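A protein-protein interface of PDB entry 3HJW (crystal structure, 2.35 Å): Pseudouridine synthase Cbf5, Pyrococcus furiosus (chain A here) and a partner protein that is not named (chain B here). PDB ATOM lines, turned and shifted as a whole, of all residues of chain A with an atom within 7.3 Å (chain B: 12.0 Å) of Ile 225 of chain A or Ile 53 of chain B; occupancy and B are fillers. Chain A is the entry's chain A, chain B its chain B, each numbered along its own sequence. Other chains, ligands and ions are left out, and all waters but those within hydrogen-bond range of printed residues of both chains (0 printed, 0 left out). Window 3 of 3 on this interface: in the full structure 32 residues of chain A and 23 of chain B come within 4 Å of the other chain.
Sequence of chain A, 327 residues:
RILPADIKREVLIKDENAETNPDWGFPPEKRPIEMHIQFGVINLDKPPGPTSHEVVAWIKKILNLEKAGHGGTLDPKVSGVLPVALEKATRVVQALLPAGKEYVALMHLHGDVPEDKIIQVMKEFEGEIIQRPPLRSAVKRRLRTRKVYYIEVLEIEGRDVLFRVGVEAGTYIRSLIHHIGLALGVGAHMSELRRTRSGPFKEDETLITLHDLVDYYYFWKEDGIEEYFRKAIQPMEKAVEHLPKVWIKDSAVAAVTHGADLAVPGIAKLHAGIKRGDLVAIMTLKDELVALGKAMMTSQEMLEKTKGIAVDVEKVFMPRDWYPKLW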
ATOM      1  N   TYR A 216      -6.567   2.188  -6.919  1.00  0.00           N
ATOM      2  CA  TYR A 216      -6.240   3.352  -7.748  1.00  0.00           C
ATOM      3  C   TYR A 216      -6.744   3.200  -9.176  1.00  0.00           C
ATOM      4  O   TYR A 216      -7.071   4.192  -9.833  1.00  0.00           O
ATOM      5  CB  TYR A 216      -4.734   3.614  -7.762  1.00  0.00           C
ATOM      6  CG  TYR A 216      -4.114   4.005  -6.421  1.00  0.00           C
ATOM      7  CD1 TYR A 216      -4.904   4.276  -5.297  1.00  0.00           C
ATOM      8  CD2 TYR A 216      -2.729   4.133  -6.295  1.00  0.00           C
ATOM      9  CE1 TYR A 216      -4.329   4.644  -4.081  1.00  0.00           C
ATOM     10  CE2 TYR A 216      -2.143   4.502  -5.091  1.00  0.00           C
ATOM     11  CZ  TYR A 216      -2.945   4.755  -3.991  1.00  0.00           C
ATOM     12  OH  TYR A 216      -2.356   5.126  -2.808  1.00  0.00           O
ATOM     13  N   TYR A 217      -6.775   1.956  -9.658  1.00  0.00           N
ATOM     14  CA  TYR A 217      -7.330   1.646 -10.971  1.00  0.00           C
ATOM     15  C   TYR A 217      -8.821   2.004 -11.004  1.00  0.00           C
ATOM     16  O   TYR A 217      -9.283   2.663 -11.926  1.00  0.00           O
ATOM     17  CB  TYR A 217      -7.101   0.169 -11.329  1.00  0.00           C
ATOM     18  CG  TYR A 217      -7.715  -0.253 -12.657  1.00  0.00           C
ATOM     19  CD1 TYR A 217      -7.130   0.127 -13.872  1.00  0.00           C
ATOM     20  CD2 TYR A 217      -8.875  -1.035 -12.698  1.00  0.00           C
ATOM     21  CE1 TYR A 217      -7.677  -0.258 -15.088  1.00  0.00           C
ATOM     22  CE2 TYR A 217      -9.436  -1.433 -13.914  1.00  0.00           C
ATOM     23  CZ  TYR A 217      -8.831  -1.042 -15.108  1.00  0.00           C
ATOM     24  OH  TYR A 217      -9.387  -1.417 -16.320  1.00  0.00           O
ATOM     25  N   TYR A 218      -9.551   1.580  -9.979  1.00  0.00           N
ATOM     26  CA  TYR A 218     -10.960   1.919  -9.835  1.00  0.00           C
ATOM     27  C   TYR A 218     -11.221   3.406  -9.600  1.00  0.00           C
ATOM     28  O   TYR A 218     -12.190   3.939 -10.124  1.00  0.00           O
ATOM     29  CB  TYR A 218     -11.618   1.061  -8.754  1.00  0.00           C
ATOM     30  CG  TYR A 218     -11.785  -0.381  -9.170  1.00  0.00           C
ATOM     31  CD1 TYR A 218     -11.330  -1.419  -8.362  1.00  0.00           C
ATOM     32  CD2 TYR A 218     -12.396  -0.711 -10.388  1.00  0.00           C
ATOM     33  CE1 TYR A 218     -11.482  -2.754  -8.743  1.00  0.00           C
ATOM     34  CE2 TYR A 218     -12.556  -2.041 -10.783  1.00  0.00           C
ATOM     35  CZ  TYR A 218     -12.098  -3.057  -9.953  1.00  0.00           C
ATOM     36  OH  TYR A 218     -12.256  -4.373 -10.339  1.00  0.00           O
ATOM     37  N   PHE A 219     -10.361   4.088  -8.846  1.00  0.00           N
ATOM     38  CA  PHE A 219     -10.488   5.547  -8.730  1.00  0.00           C
ATOM     39  C   PHE A 219     -10.382   6.203 -10.111  1.00  0.00           C
ATOM     40  O   PHE A 219     -11.071   7.191 -10.389  1.00  0.00           O
ATOM     41  CB  PHE A 219      -9.451   6.159  -7.779  1.00  0.00           C
ATOM     42  CG  PHE A 219      -9.528   5.653  -6.359  1.00  0.00           C
ATOM     43  CD1 PHE A 219      -8.420   5.759  -5.522  1.00  0.00           C
ATOM     44  CD2 PHE A 219     -10.685   5.067  -5.860  1.00  0.00           C
ATOM     45  CE1 PHE A 219      -8.470   5.299  -4.199  1.00  0.00           C
ATOM     46  CE2 PHE A 219     -10.748   4.604  -4.551  1.00  0.00           C
ATOM     47  CZ  PHE A 219      -9.634   4.718  -3.714  1.00  0.00           C
ATOM     48  N   TRP A 220      -9.525   5.650 -10.973  1.00  0.00           N
ATOM     49  CA  TRP A 220      -9.398   6.160 -12.331  1.00  0.00           C
ATOM     50  C   TRP A 220     -10.601   5.754 -13.193  1.00  0.00           C
ATOM     51  O   TRP A 220     -11.325   6.611 -13.700  1.00  0.00           O
ATOM     52  CB  TRP A 220      -8.087   5.712 -12.980  1.00  0.00           C
ATOM     53  CG  TRP A 220      -8.049   5.965 -14.481  1.00  0.00           C
ATOM     54  CD1 TRP A 220      -8.433   7.108 -15.134  1.00  0.00           C
ATOM     55  CD2 TRP A 220      -7.597   5.059 -15.499  1.00  0.00           C
ATOM     56  NE1 TRP A 220      -8.257   6.961 -16.492  1.00  0.00           N
ATOM     57  CE2 TRP A 220      -7.743   5.718 -16.742  1.00  0.00           C
ATOM     58  CE3 TRP A 220      -7.085   3.755 -15.482  1.00  0.00           C
ATOM     59  CZ2 TRP A 220      -7.395   5.118 -17.956  1.00  0.00           C
ATOM     60  CZ3 TRP A 220      -6.742   3.157 -16.689  1.00  0.00           C
ATOM     61  CH2 TRP A 220      -6.898   3.840 -17.910  1.00  0.00           C
ATOM     62  N   LYS A 221     -10.792   4.444 -13.344  1.00  0.00           N
ATOM     63  CA  LYS A 221     -11.832   3.869 -14.195  1.00  0.00           C
ATOM     64  C   LYS A 221     -13.234   4.324 -13.809  1.00  0.00           C
ATOM     65  O   LYS A 221     -14.025   4.726 -14.673  1.00  0.00           O
ATOM     66  CB  LYS A 221     -11.748   2.335 -14.149  1.00  0.00           C
ATOM     67  CG  LYS A 221     -11.164   1.659 -15.393  1.00  0.00           C
ATOM     68  CD  LYS A 221     -10.536   2.652 -16.355  1.00  0.00           C
ATOM     69  CE  LYS A 221     -10.229   2.015 -17.694  1.00  0.00           C
ATOM     70  NZ  LYS A 221     -11.422   1.549 -18.431  1.00  0.00           N
ATOM     71  N   GLU A 222     -13.526   4.279 -12.513  1.00  0.00           N
ATOM     72  CA  GLU A 222     -14.893   4.467 -12.027  1.00  0.00           C
ATOM     73  C   GLU A 222     -15.199   5.826 -11.387  1.00  0.00           C
ATOM     74  O   GLU A 222     -16.366   6.213 -11.312  1.00  0.00           O
ATOM     75  CB  GLU A 222     -15.287   3.314 -11.092  1.00  0.00           C
ATOM     76  CG  GLU A 222     -15.525   2.002 -11.838  1.00  0.00           C
ATOM     77  CD  GLU A 222     -15.819   0.821 -10.927  1.00  0.00           C
ATOM     78  OE1 GLU A 222     -16.030  -0.292 -11.459  1.00  0.00           O
ATOM     79  OE2 GLU A 222     -15.832   0.992  -9.690  1.00  0.00           O
ATOM     80  N   ASP A 223     -14.160   6.536 -10.947  1.00  0.00           N
ATOM     81  CA  ASP A 223     -14.307   7.855 -10.317  1.00  0.00           C
ATOM     82  C   ASP A 223     -13.772   8.978 -11.204  1.00  0.00           C
ATOM     83  O   ASP A 223     -14.032  10.155 -10.946  1.00  0.00           O
ATOM     84  CB  ASP A 223     -13.577   7.904  -8.965  1.00  0.00           C
ATOM     85  CG  ASP A 223     -14.119   6.907  -7.953  1.00  0.00           C
ATOM     86  OD1 ASP A 223     -14.113   7.240  -6.748  1.00  0.00           O
ATOM     87  OD2 ASP A 223     -14.544   5.796  -8.344  1.00  0.00           O
ATOM     88  N   GLY A 224     -13.008   8.616 -12.232  1.00  0.00           N
ATOM     89  CA  GLY A 224     -12.426   9.598 -13.148  1.00  0.00           C
ATOM     90  C   GLY A 224     -11.201  10.327 -12.616  1.00  0.00           C
ATOM     91  O   GLY A 224     -10.790  11.342 -13.191  1.00  0.00           O
ATOM     92  N   ILE A 225     -10.615   9.820 -11.529  1.00  0.00           N
ATOM     93  CA  ILE A 225      -9.408  10.423 -10.942  1.00  0.00           C
ATOM     94  C   ILE A 225      -8.136   9.732 -11.444  1.00  0.00           C
ATOM     95  O   ILE A 225      -7.847   8.594 -11.074  1.00  0.00           O
ATOM     96  CB  ILE A 225      -9.418  10.404  -9.385  1.00  0.00           C
ATOM     97  CG1 ILE A 225     -10.723  10.987  -8.815  1.00  0.00           C
ATOM     98  CG2 ILE A 225      -8.172  11.114  -8.824  1.00  0.00           C
ATOM     99  CD1 ILE A 225     -10.932  12.486  -9.070  1.00  0.00           C
ATOM    100  N   GLU A 226      -7.372  10.447 -12.265  1.00  0.00           N
ATOM    101  CA  GLU A 226      -6.207   9.894 -12.959  1.00  0.00           C
ATOM    102  C   GLU A 226      -4.921   9.820 -12.094  1.00  0.00           C
ATOM    103  O   GLU A 226      -4.109   8.909 -12.271  1.00  0.00           O
ATOM    104  CB  GLU A 226      -5.956  10.719 -14.224  1.00  0.00           C
ATOM    105  CG  GLU A 226      -5.138  10.042 -15.299  1.00  0.00           C
ATOM    106  CD  GLU A 226      -4.803  10.982 -16.454  1.00  0.00           C
ATOM    107  OE1 GLU A 226      -5.730  11.368 -17.212  1.00  0.00           O
ATOM    108  OE2 GLU A 226      -3.603  11.328 -16.604  1.00  0.00           O
ATOM    109  N   GLU A 227      -4.767  10.773 -11.170  1.00  0.00           N
ATOM    110  CA  GLU A 227      -3.548  10.978 -10.367  1.00  0.00           C
ATOM    111  C   GLU A 227      -2.908   9.741  -9.741  1.00  0.00           C
ATOM    112  O   GLU A 227      -1.703   9.516  -9.888  1.00  0.00           O
ATOM    113  CB  GLU A 227      -3.823  11.966  -9.232  1.00  0.00           C
ATOM    114  CG  GLU A 227      -3.532  13.421  -9.555  1.00  0.00           C
ATOM    115  CD  GLU A 227      -3.895  14.357  -8.396  1.00  0.00           C
ATOM    116  OE1 GLU A 227      -3.584  14.016  -7.225  1.00  0.00           O
ATOM    117  OE2 GLU A 227      -4.494  15.430  -8.666  1.00  0.00           O
ATOM    118  N   TYR A 228      -3.713   8.968  -9.018  1.00  0.00           N
ATOM    119  CA  TYR A 228      -3.190   7.881  -8.203  1.00  0.00           C
ATOM    120  C   TYR A 228      -2.691   6.705  -9.039  1.00  0.00           C
ATOM    121  O   TYR A 228      -1.575   6.220  -8.836  1.00  0.00           O
ATOM    122  CB  TYR A 228      -4.227   7.444  -7.162  1.00  0.00           C
ATOM    123  CG  TYR A 228      -4.575   8.560  -6.214  1.00  0.00           C
ATOM    124  CD1 TYR A 228      -5.740   9.314  -6.388  1.00  0.00           C
ATOM    125  CD2 TYR A 228      -3.716   8.897  -5.161  1.00  0.00           C
ATOM    126  CE1 TYR A 228      -6.050  10.363  -5.524  1.00  0.00           C
ATOM    127  CE2 TYR A 228      -4.012   9.942  -4.298  1.00  0.00           C
ATOM    128  CZ  TYR A 228      -5.178  10.669  -4.482  1.00  0.00           C
ATOM    129  OH  TYR A 228      -5.471  11.692  -3.611  1.00  0.00           O
ATOM    130  N   PHE A 229      -3.517   6.262  -9.979  1.00  0.00           N
ATOM    131  CA  PHE A 229      -3.153   5.152 -10.844  1.00  0.00           C
ATOM    132  C   PHE A 229      -1.966   5.538 -11.704  1.00  0.00           C
ATOM    133  O   PHE A 229      -1.129   4.693 -12.025  1.00  0.00           O
ATOM    134  CB  PHE A 229      -4.335   4.719 -11.706  1.00  0.00           C
ATOM    135  CG  PHE A 229      -4.091   3.459 -12.474  1.00  0.00           C
ATOM    136  CD1 PHE A 229      -3.954   2.246 -11.815  1.00  0.00           C
ATOM    137  CD2 PHE A 229      -3.988   3.491 -13.853  1.00  0.00           C
ATOM    138  CE1 PHE A 229      -3.729   1.074 -12.528  1.00  0.00           C
ATOM    139  CE2 PHE A 229      -3.764   2.329 -14.582  1.00  0.00           C
ATOM    140  CZ  PHE A 229      -3.635   1.119 -13.922  1.00  0.00           C
ATOM    141  N   ARG A 230      -1.889   6.823 -12.047  1.00  0.00           N
ATOM    142  CA  ARG A 230      -0.757   7.356 -12.808  1.00  0.00           C
ATOM    143  C   ARG A 230       0.573   7.152 -12.073  1.00  0.00           C
ATOM    144  O   ARG A 230       1.552   6.717 -12.676  1.00  0.00           O
ATOM    145  CB  ARG A 230      -0.969   8.829 -13.166  1.00  0.00           C
ATOM    146  CG  ARG A 230       0.065   9.322 -14.135  1.00  0.00           C
ATOM    147  CD  ARG A 230      -0.296  10.623 -14.815  1.00  0.00           C
ATOM    148  NE  ARG A 230       0.689  10.859 -15.860  1.00  0.00           N
ATOM    149  CZ  ARG A 230       0.461  10.777 -17.167  1.00  0.00           C
ATOM    150  NH1 ARG A 230      -0.754  10.516 -17.648  1.00  0.00           N
ATOM    151  NH2 ARG A 230       1.465  10.989 -18.000  1.00  0.00           N
ATOM    152  N   GLY B  40     -13.524  -4.901  -1.421  1.00  0.00           N
ATOM    153  CA  GLY B  40     -12.861  -3.822  -2.145  1.00  0.00           C
ATOM    154  C   GLY B  40     -13.681  -2.547  -2.119  1.00  0.00           C
ATOM    155  O   GLY B  40     -13.163  -1.473  -1.829  1.00  0.00           O
ATOM    156  N   GLU B  41     -14.971  -2.688  -2.401  1.00  0.00           N
ATOM    157  CA  GLU B  41     -15.922  -1.580  -2.391  1.00  0.00           C
ATOM    158  C   GLU B  41     -15.904  -0.801  -1.067  1.00  0.00           C
ATOM    159  O   GLU B  41     -15.793   0.427  -1.061  1.00  0.00           O
ATOM    160  CB  GLU B  41     -17.323  -2.124  -2.676  1.00  0.00           C
ATOM    161  CG  GLU B  41     -18.381  -1.065  -2.910  1.00  0.00           C
ATOM    162  CD  GLU B  41     -19.784  -1.584  -2.651  1.00  0.00           C
ATOM    163  OE1 GLU B  41     -19.982  -2.824  -2.661  1.00  0.00           O
ATOM    164  OE2 GLU B  41     -20.692  -0.749  -2.438  1.00  0.00           O
ATOM    165  N   TYR B  42     -15.991  -1.528   0.041  1.00  0.00           N
ATOM    166  CA  TYR B  42     -16.012  -0.930   1.368  1.00  0.00           C
ATOM    167  C   TYR B  42     -14.641  -0.458   1.830  1.00  0.00           C
ATOM    168  O   TYR B  42     -14.532   0.578   2.492  1.00  0.00           O
ATOM    169  CB  TYR B  42     -16.672  -1.882   2.370  1.00  0.00           C
ATOM    170  CG  TYR B  42     -18.136  -2.081   2.037  1.00  0.00           C
ATOM    171  CD1 TYR B  42     -18.561  -3.184   1.287  1.00  0.00           C
ATOM    172  CD2 TYR B  42     -19.091  -1.136   2.422  1.00  0.00           C
ATOM    173  CE1 TYR B  42     -19.911  -3.355   0.953  1.00  0.00           C
ATOM    174  CE2 TYR B  42     -20.436  -1.296   2.098  1.00  0.00           C
ATOM    175  CZ  TYR B  42     -20.841  -2.406   1.362  1.00  0.00           C
ATOM    176  OH  TYR B  42     -22.177  -2.564   1.041  1.00  0.00           O
ATOM    177  N   ARG B  43     -13.603  -1.211   1.472  1.00  0.00           N
ATOM    178  CA  ARG B  43     -12.229  -0.772   1.678  1.00  0.00           C
ATOM    179  C   ARG B  43     -11.966   0.515   0.890  1.00  0.00           C
ATOM    180  O   ARG B  43     -11.357   1.453   1.414  1.00  0.00           O
ATOM    181  CB  ARG B  43     -11.230  -1.869   1.289  1.00  0.00           C
ATOM    182  CG  ARG B  43      -9.772  -1.445   1.396  1.00  0.00           C
ATOM    183  CD  ARG B  43      -8.802  -2.457   0.787  1.00  0.00           C
ATOM    184  NE  ARG B  43      -8.823  -2.467  -0.677  1.00  0.00           N
ATOM    185  CZ  ARG B  43      -9.145  -3.526  -1.420  1.00  0.00           C
ATOM    186  NH1 ARG B  43      -9.467  -4.679  -0.849  1.00  0.00           N
ATOM    187  NH2 ARG B  43      -9.130  -3.436  -2.746  1.00  0.00           N
ATOM    188  N   ARG B  44     -12.438   0.562  -0.353  1.00  0.00           N
ATOM    189  CA  ARG B  44     -12.333   1.774  -1.175  1.00  0.00           C
ATOM    190  C   ARG B  44     -13.025   2.994  -0.567  1.00  0.00           C
ATOM    191  O   ARG B  44     -12.563   4.114  -0.753  1.00  0.00           O
ATOM    192  CB  ARG B  44     -12.854   1.530  -2.589  1.00  0.00           C
ATOM    193  CG  ARG B  44     -11.763   1.360  -3.618  1.00  0.00           C
ATOM    194  CD  ARG B  44     -12.306   0.933  -4.972  1.00  0.00           C
ATOM    195  NE  ARG B  44     -12.094  -0.496  -5.174  1.00  0.00           N
ATOM    196  CZ  ARG B  44     -13.055  -1.404  -5.256  1.00  0.00           C
ATOM    197  NH1 ARG B  44     -14.320  -1.039  -5.181  1.00  0.00           N
ATOM    198  NH2 ARG B  44     -12.747  -2.680  -5.424  1.00  0.00           N
ATOM    199  N   ARG B  45     -14.119   2.771   0.156  1.00  0.00           N
ATOM    200  CA  ARG B  45     -14.847   3.860   0.811  1.00  0.00           C
ATOM    201  C   ARG B  45     -14.047   4.450   1.977  1.00  0.00           C
ATOM    202  O   ARG B  45     -14.051   5.663   2.195  1.00  0.00           O
ATOM    203  CB  ARG B  45     -16.233   3.393   1.274  1.00  0.00           C
ATOM    204  CG  ARG B  45     -17.249   4.523   1.382  1.00  0.00           C
ATOM    205  CD  ARG B  45     -18.703   4.028   1.486  1.00  0.00           C
ATOM    206  NE  ARG B  45     -19.031   3.042   0.450  1.00  0.00           N
ATOM    207  CZ  ARG B  45     -20.164   2.342   0.390  1.00  0.00           C
ATOM    208  NH1 ARG B  45     -21.128   2.510   1.292  1.00  0.00           N
ATOM    209  NH2 ARG B  45     -20.333   1.469  -0.593  1.00  0.00           N
ATOM    210  N   TRP B  46     -13.361   3.574   2.709  1.00  0.00           N
ATOM    211  CA  TRP B  46     -12.423   3.969   3.763  1.00  0.00           C
ATOM    212  C   TRP B  46     -11.240   4.738   3.178  1.00  0.00           C
ATOM    213  O   TRP B  46     -10.881   5.805   3.681  1.00  0.00           O
ATOM    214  CB  TRP B  46     -11.945   2.721   4.515  1.00  0.00           C
ATOM    215  CG  TRP B  46     -10.633   2.846   5.235  1.00  0.00           C
ATOM    216  CD1 TRP B  46     -10.380   3.564   6.374  1.00  0.00           C
ATOM    217  CD2 TRP B  46      -9.403   2.197   4.892  1.00  0.00           C
ATOM    218  NE1 TRP B  46      -9.070   3.412   6.750  1.00  0.00           N
ATOM    219  CE2 TRP B  46      -8.444   2.582   5.858  1.00  0.00           C
ATOM    220  CE3 TRP B  46      -9.015   1.329   3.858  1.00  0.00           C
ATOM    221  CZ2 TRP B  46      -7.113   2.132   5.820  1.00  0.00           C
ATOM    222  CZ3 TRP B  46      -7.684   0.881   3.816  1.00  0.00           C
ATOM    223  CH2 TRP B  46      -6.754   1.286   4.795  1.00  0.00           C
ATOM    224  N   LYS B  47     -10.671   4.195   2.098  1.00  0.00           N
ATOM    225  CA  LYS B  47      -9.500   4.770   1.431  1.00  0.00           C
ATOM    226  C   LYS B  47      -9.791   6.130   0.800  1.00  0.00           C
ATOM    227  O   LYS B  47      -8.922   7.011   0.802  1.00  0.00           O
ATOM    228  CB  LYS B  47      -8.949   3.803   0.372  1.00  0.00           C
ATOM    229  CG  LYS B  47      -7.527   4.124  -0.077  1.00  0.00           C
ATOM    230  CD  LYS B  47      -6.895   2.987  -0.873  1.00  0.00           C
ATOM    231  CE  LYS B  47      -6.549   1.769  -0.002  1.00  0.00           C
ATOM    232  NZ  LYS B  47      -5.974   0.669  -0.839  1.00  0.00           N
ATOM    233  N   ARG B  48     -11.003   6.286   0.260  1.00  0.00           N
ATOM    234  CA  ARG B  48     -11.451   7.568  -0.298  1.00  0.00           C
ATOM    235  C   ARG B  48     -11.530   8.638   0.786  1.00  0.00           C
ATOM    236  O   ARG B  48     -11.148   9.783   0.554  1.00  0.00           O
ATOM    237  CB  ARG B  48     -12.799   7.435  -1.017  1.00  0.00           C
ATOM    238  CG  ARG B  48     -12.711   6.841  -2.418  1.00  0.00           C
ATOM    239  CD  ARG B  48     -14.040   6.915  -3.159  1.00  0.00           C
ATOM    240  NE  ARG B  48     -14.087   5.992  -4.296  1.00  0.00           N
ATOM    241  CZ  ARG B  48     -14.653   4.785  -4.264  1.00  0.00           C
ATOM    242  NH1 ARG B  48     -15.233   4.341  -3.157  1.00  0.00           N
ATOM    243  NH2 ARG B  48     -14.634   4.016  -5.340  1.00  0.00           N
ATOM    244  N   GLU B  49     -12.011   8.257   1.967  1.00  0.00           N
ATOM    245  CA  GLU B  49     -12.062   9.153   3.117  1.00  0.00           C
ATOM    246  C   GLU B  49     -10.651   9.563   3.579  1.00  0.00           C
ATOM    247  O   GLU B  49     -10.415  10.713   3.957  1.00  0.00           O
ATOM    248  CB  GLU B  49     -12.854   8.499   4.260  1.00  0.00           C
ATOM    249  CG  GLU B  49     -13.166   9.427   5.434  1.00  0.00           C
ATOM    250  CD  GLU B  49     -14.258   8.894   6.362  1.00  0.00           C
ATOM    251  OE1 GLU B  49     -15.388   8.632   5.884  1.00  0.00           O
ATOM    252  OE2 GLU B  49     -13.989   8.761   7.582  1.00  0.00           O
ATOM    253  N   VAL B  50      -9.720   8.617   3.526  1.00  0.00           N
ATOM    254  CA  VAL B  50      -8.336   8.850   3.927  1.00  0.00           C
ATOM    255  C   VAL B  50      -7.598   9.795   2.964  1.00  0.00           C
ATOM    256  O   VAL B  50      -6.760  10.596   3.394  1.00  0.00           O
ATOM    257  CB  VAL B  50      -7.579   7.498   4.096  1.00  0.00           C
ATOM    258  CG1 VAL B  50      -6.056   7.688   4.157  1.00  0.00           C
ATOM    259  CG2 VAL B  50      -8.083   6.760   5.334  1.00  0.00           C
ATOM    260  N   LEU B  51      -7.913   9.693   1.676  1.00  0.00           N
ATOM    261  CA  LEU B  51      -7.084  10.288   0.635  1.00  0.00           C
ATOM    262  C   LEU B  51      -7.553  11.699   0.296  1.00  0.00           C
ATOM    263  O   LEU B  51      -6.953  12.380  -0.536  1.00  0.00           O
ATOM    264  CB  LEU B  51      -7.094   9.415  -0.621  1.00  0.00           C
ATOM    265  CG  LEU B  51      -6.167   8.198  -0.608  1.00  0.00           C
ATOM    266  CD1 LEU B  51      -6.293   7.413  -1.905  1.00  0.00           C
ATOM    267  CD2 LEU B  51      -4.726   8.622  -0.371  1.00  0.00           C
ATOM    268  N   GLY B  52      -8.629  12.132   0.946  1.00  0.00           N
ATOM    269  CA  GLY B  52      -9.204  13.437   0.683  1.00  0.00           C
ATOM    270  C   GLY B  52      -9.916  13.499  -0.655  1.00  0.00           C
ATOM    271  O   GLY B  52     -10.187  14.581  -1.175  1.00  0.00           O
ATOM    272  N   ILE B  53     -10.221  12.332  -1.211  1.00  0.00           N
ATOM    273  CA  ILE B  53     -10.826  12.249  -2.535  1.00  0.00           C
ATOM    274  C   ILE B  53     -12.348  12.211  -2.445  1.00  0.00           C
ATOM    275  O   ILE B  53     -12.950  12.928  -1.647  1.00  0.00           O
ATOM    276  CB  ILE B  53     -10.336  11.007  -3.303  1.00  0.00           C
ATOM    277  CG1 ILE B  53     -10.872  11.019  -4.736  1.00  0.00           C
ATOM    278  CG2 ILE B  53     -10.756   9.734  -2.583  1.00  0.00           C
ATOM    279  CD1 ILE B  53     -10.371  12.183  -5.565  1.00  0.00           C
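Of the 15 printed residues of chain A, 5 touch a printed residue of chain B. Hydrophobic or aromatic side chains of chain B within 4 Å of the printed part of chain A: Leu 51 and Ile 53. Along chain B the printed residues that touch a printed residue of chain A span positions 44 to 53. Among the printed residues, 7 pairs touch across the chains. Among the printed residues, Asp or Glu carboxylates within 4 Å of a Lys or Arg side-chain nitrogen of the other chain: Asp 223 of chain A with Arg 48 of chain B (2.8 Å).
The side-chain carboxylate of Asp 223 of chain A is in salt-bridge range of the guanidinium group of Arg 48 of chain B, at 2.8 Å. The side-chain hydroxyl (OH) of Tyr 228 of chain A sits at hydrogen-bond distance from the backbone carbonyl oxygen (O) of Leu 51 of chain B.
Ile 225 of chain A touches just one residue of chain B: Ile 53 (3.5 Å). Of chain A, only Ile 225 comes within 4 Å of Ile 53 of chain B. Phe 219 of chain A touches three residues of chain B. Asp 223 of chain A touches just one residue of chain B: Arg 48 (2.8 Å). Gly 224 of chain A touches none of the printed residues of chain B. No residue of chain B comes within 4 Å of Glu 226 of chain A. No residue of chain A comes within 4 Å of Gly 52 of chain B. Of the printed residues of chain A, Leu 51 of chain B touches Phe 219 and Tyr 228. Of the printed residues of chain A, Arg 44 of chain B touches Tyr 218 (3.4 Å) and Phe 219 (3.5 Å). Arg 230 of chain A touches none of the printed residues of chain B. The nearest residue of chain B that does not touch Ile 225 of chain A is Arg 48 of chain B (7.5 Å). The nearest residue of chain A that does not touch Ile 53 of chain B is Tyr 228 of chain A (4.7 Å).
CD1 of Tyr 218 of chain A touches NE of Arg 44 of chain B, at 3.4 Å. Arg 44 of chain B touches Phe 219 of chain A (CG to CE2, 3.5 Å). CE2 of Phe 219 of chain A touches NE of Arg 48 of chain B (3.6 Å). CD1 of Leu 51 of chain B touches CE1 of Phe 219 of chain A (3.8 Å). CG1 of Ile 225 of chain A touches CD1 of Ile 53 of chain B (3.5 Å).
O of Tyr 218 of chain A lies within hydrogen-bond range of N of Asp 223 of chain A (3.4 Å). The backbone carbonyl oxygen (O) of Phe 219 of chain A lies within hydrogen-bond range of the backbone NH (N) of Gly 224 of chain A, at 3.0 Å. O of Phe 219 of chain A is in hydrogen-bond range of N of Ile 225 of chain A. O of Ile 225 of chain A sits close to N of Trp 220 of chain A, at 3.4 Å. The backbone carbonyl oxygen of Arg 48 of chain B lies close to the backbone NH of Ile 53 of chain B (3.2 Å).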
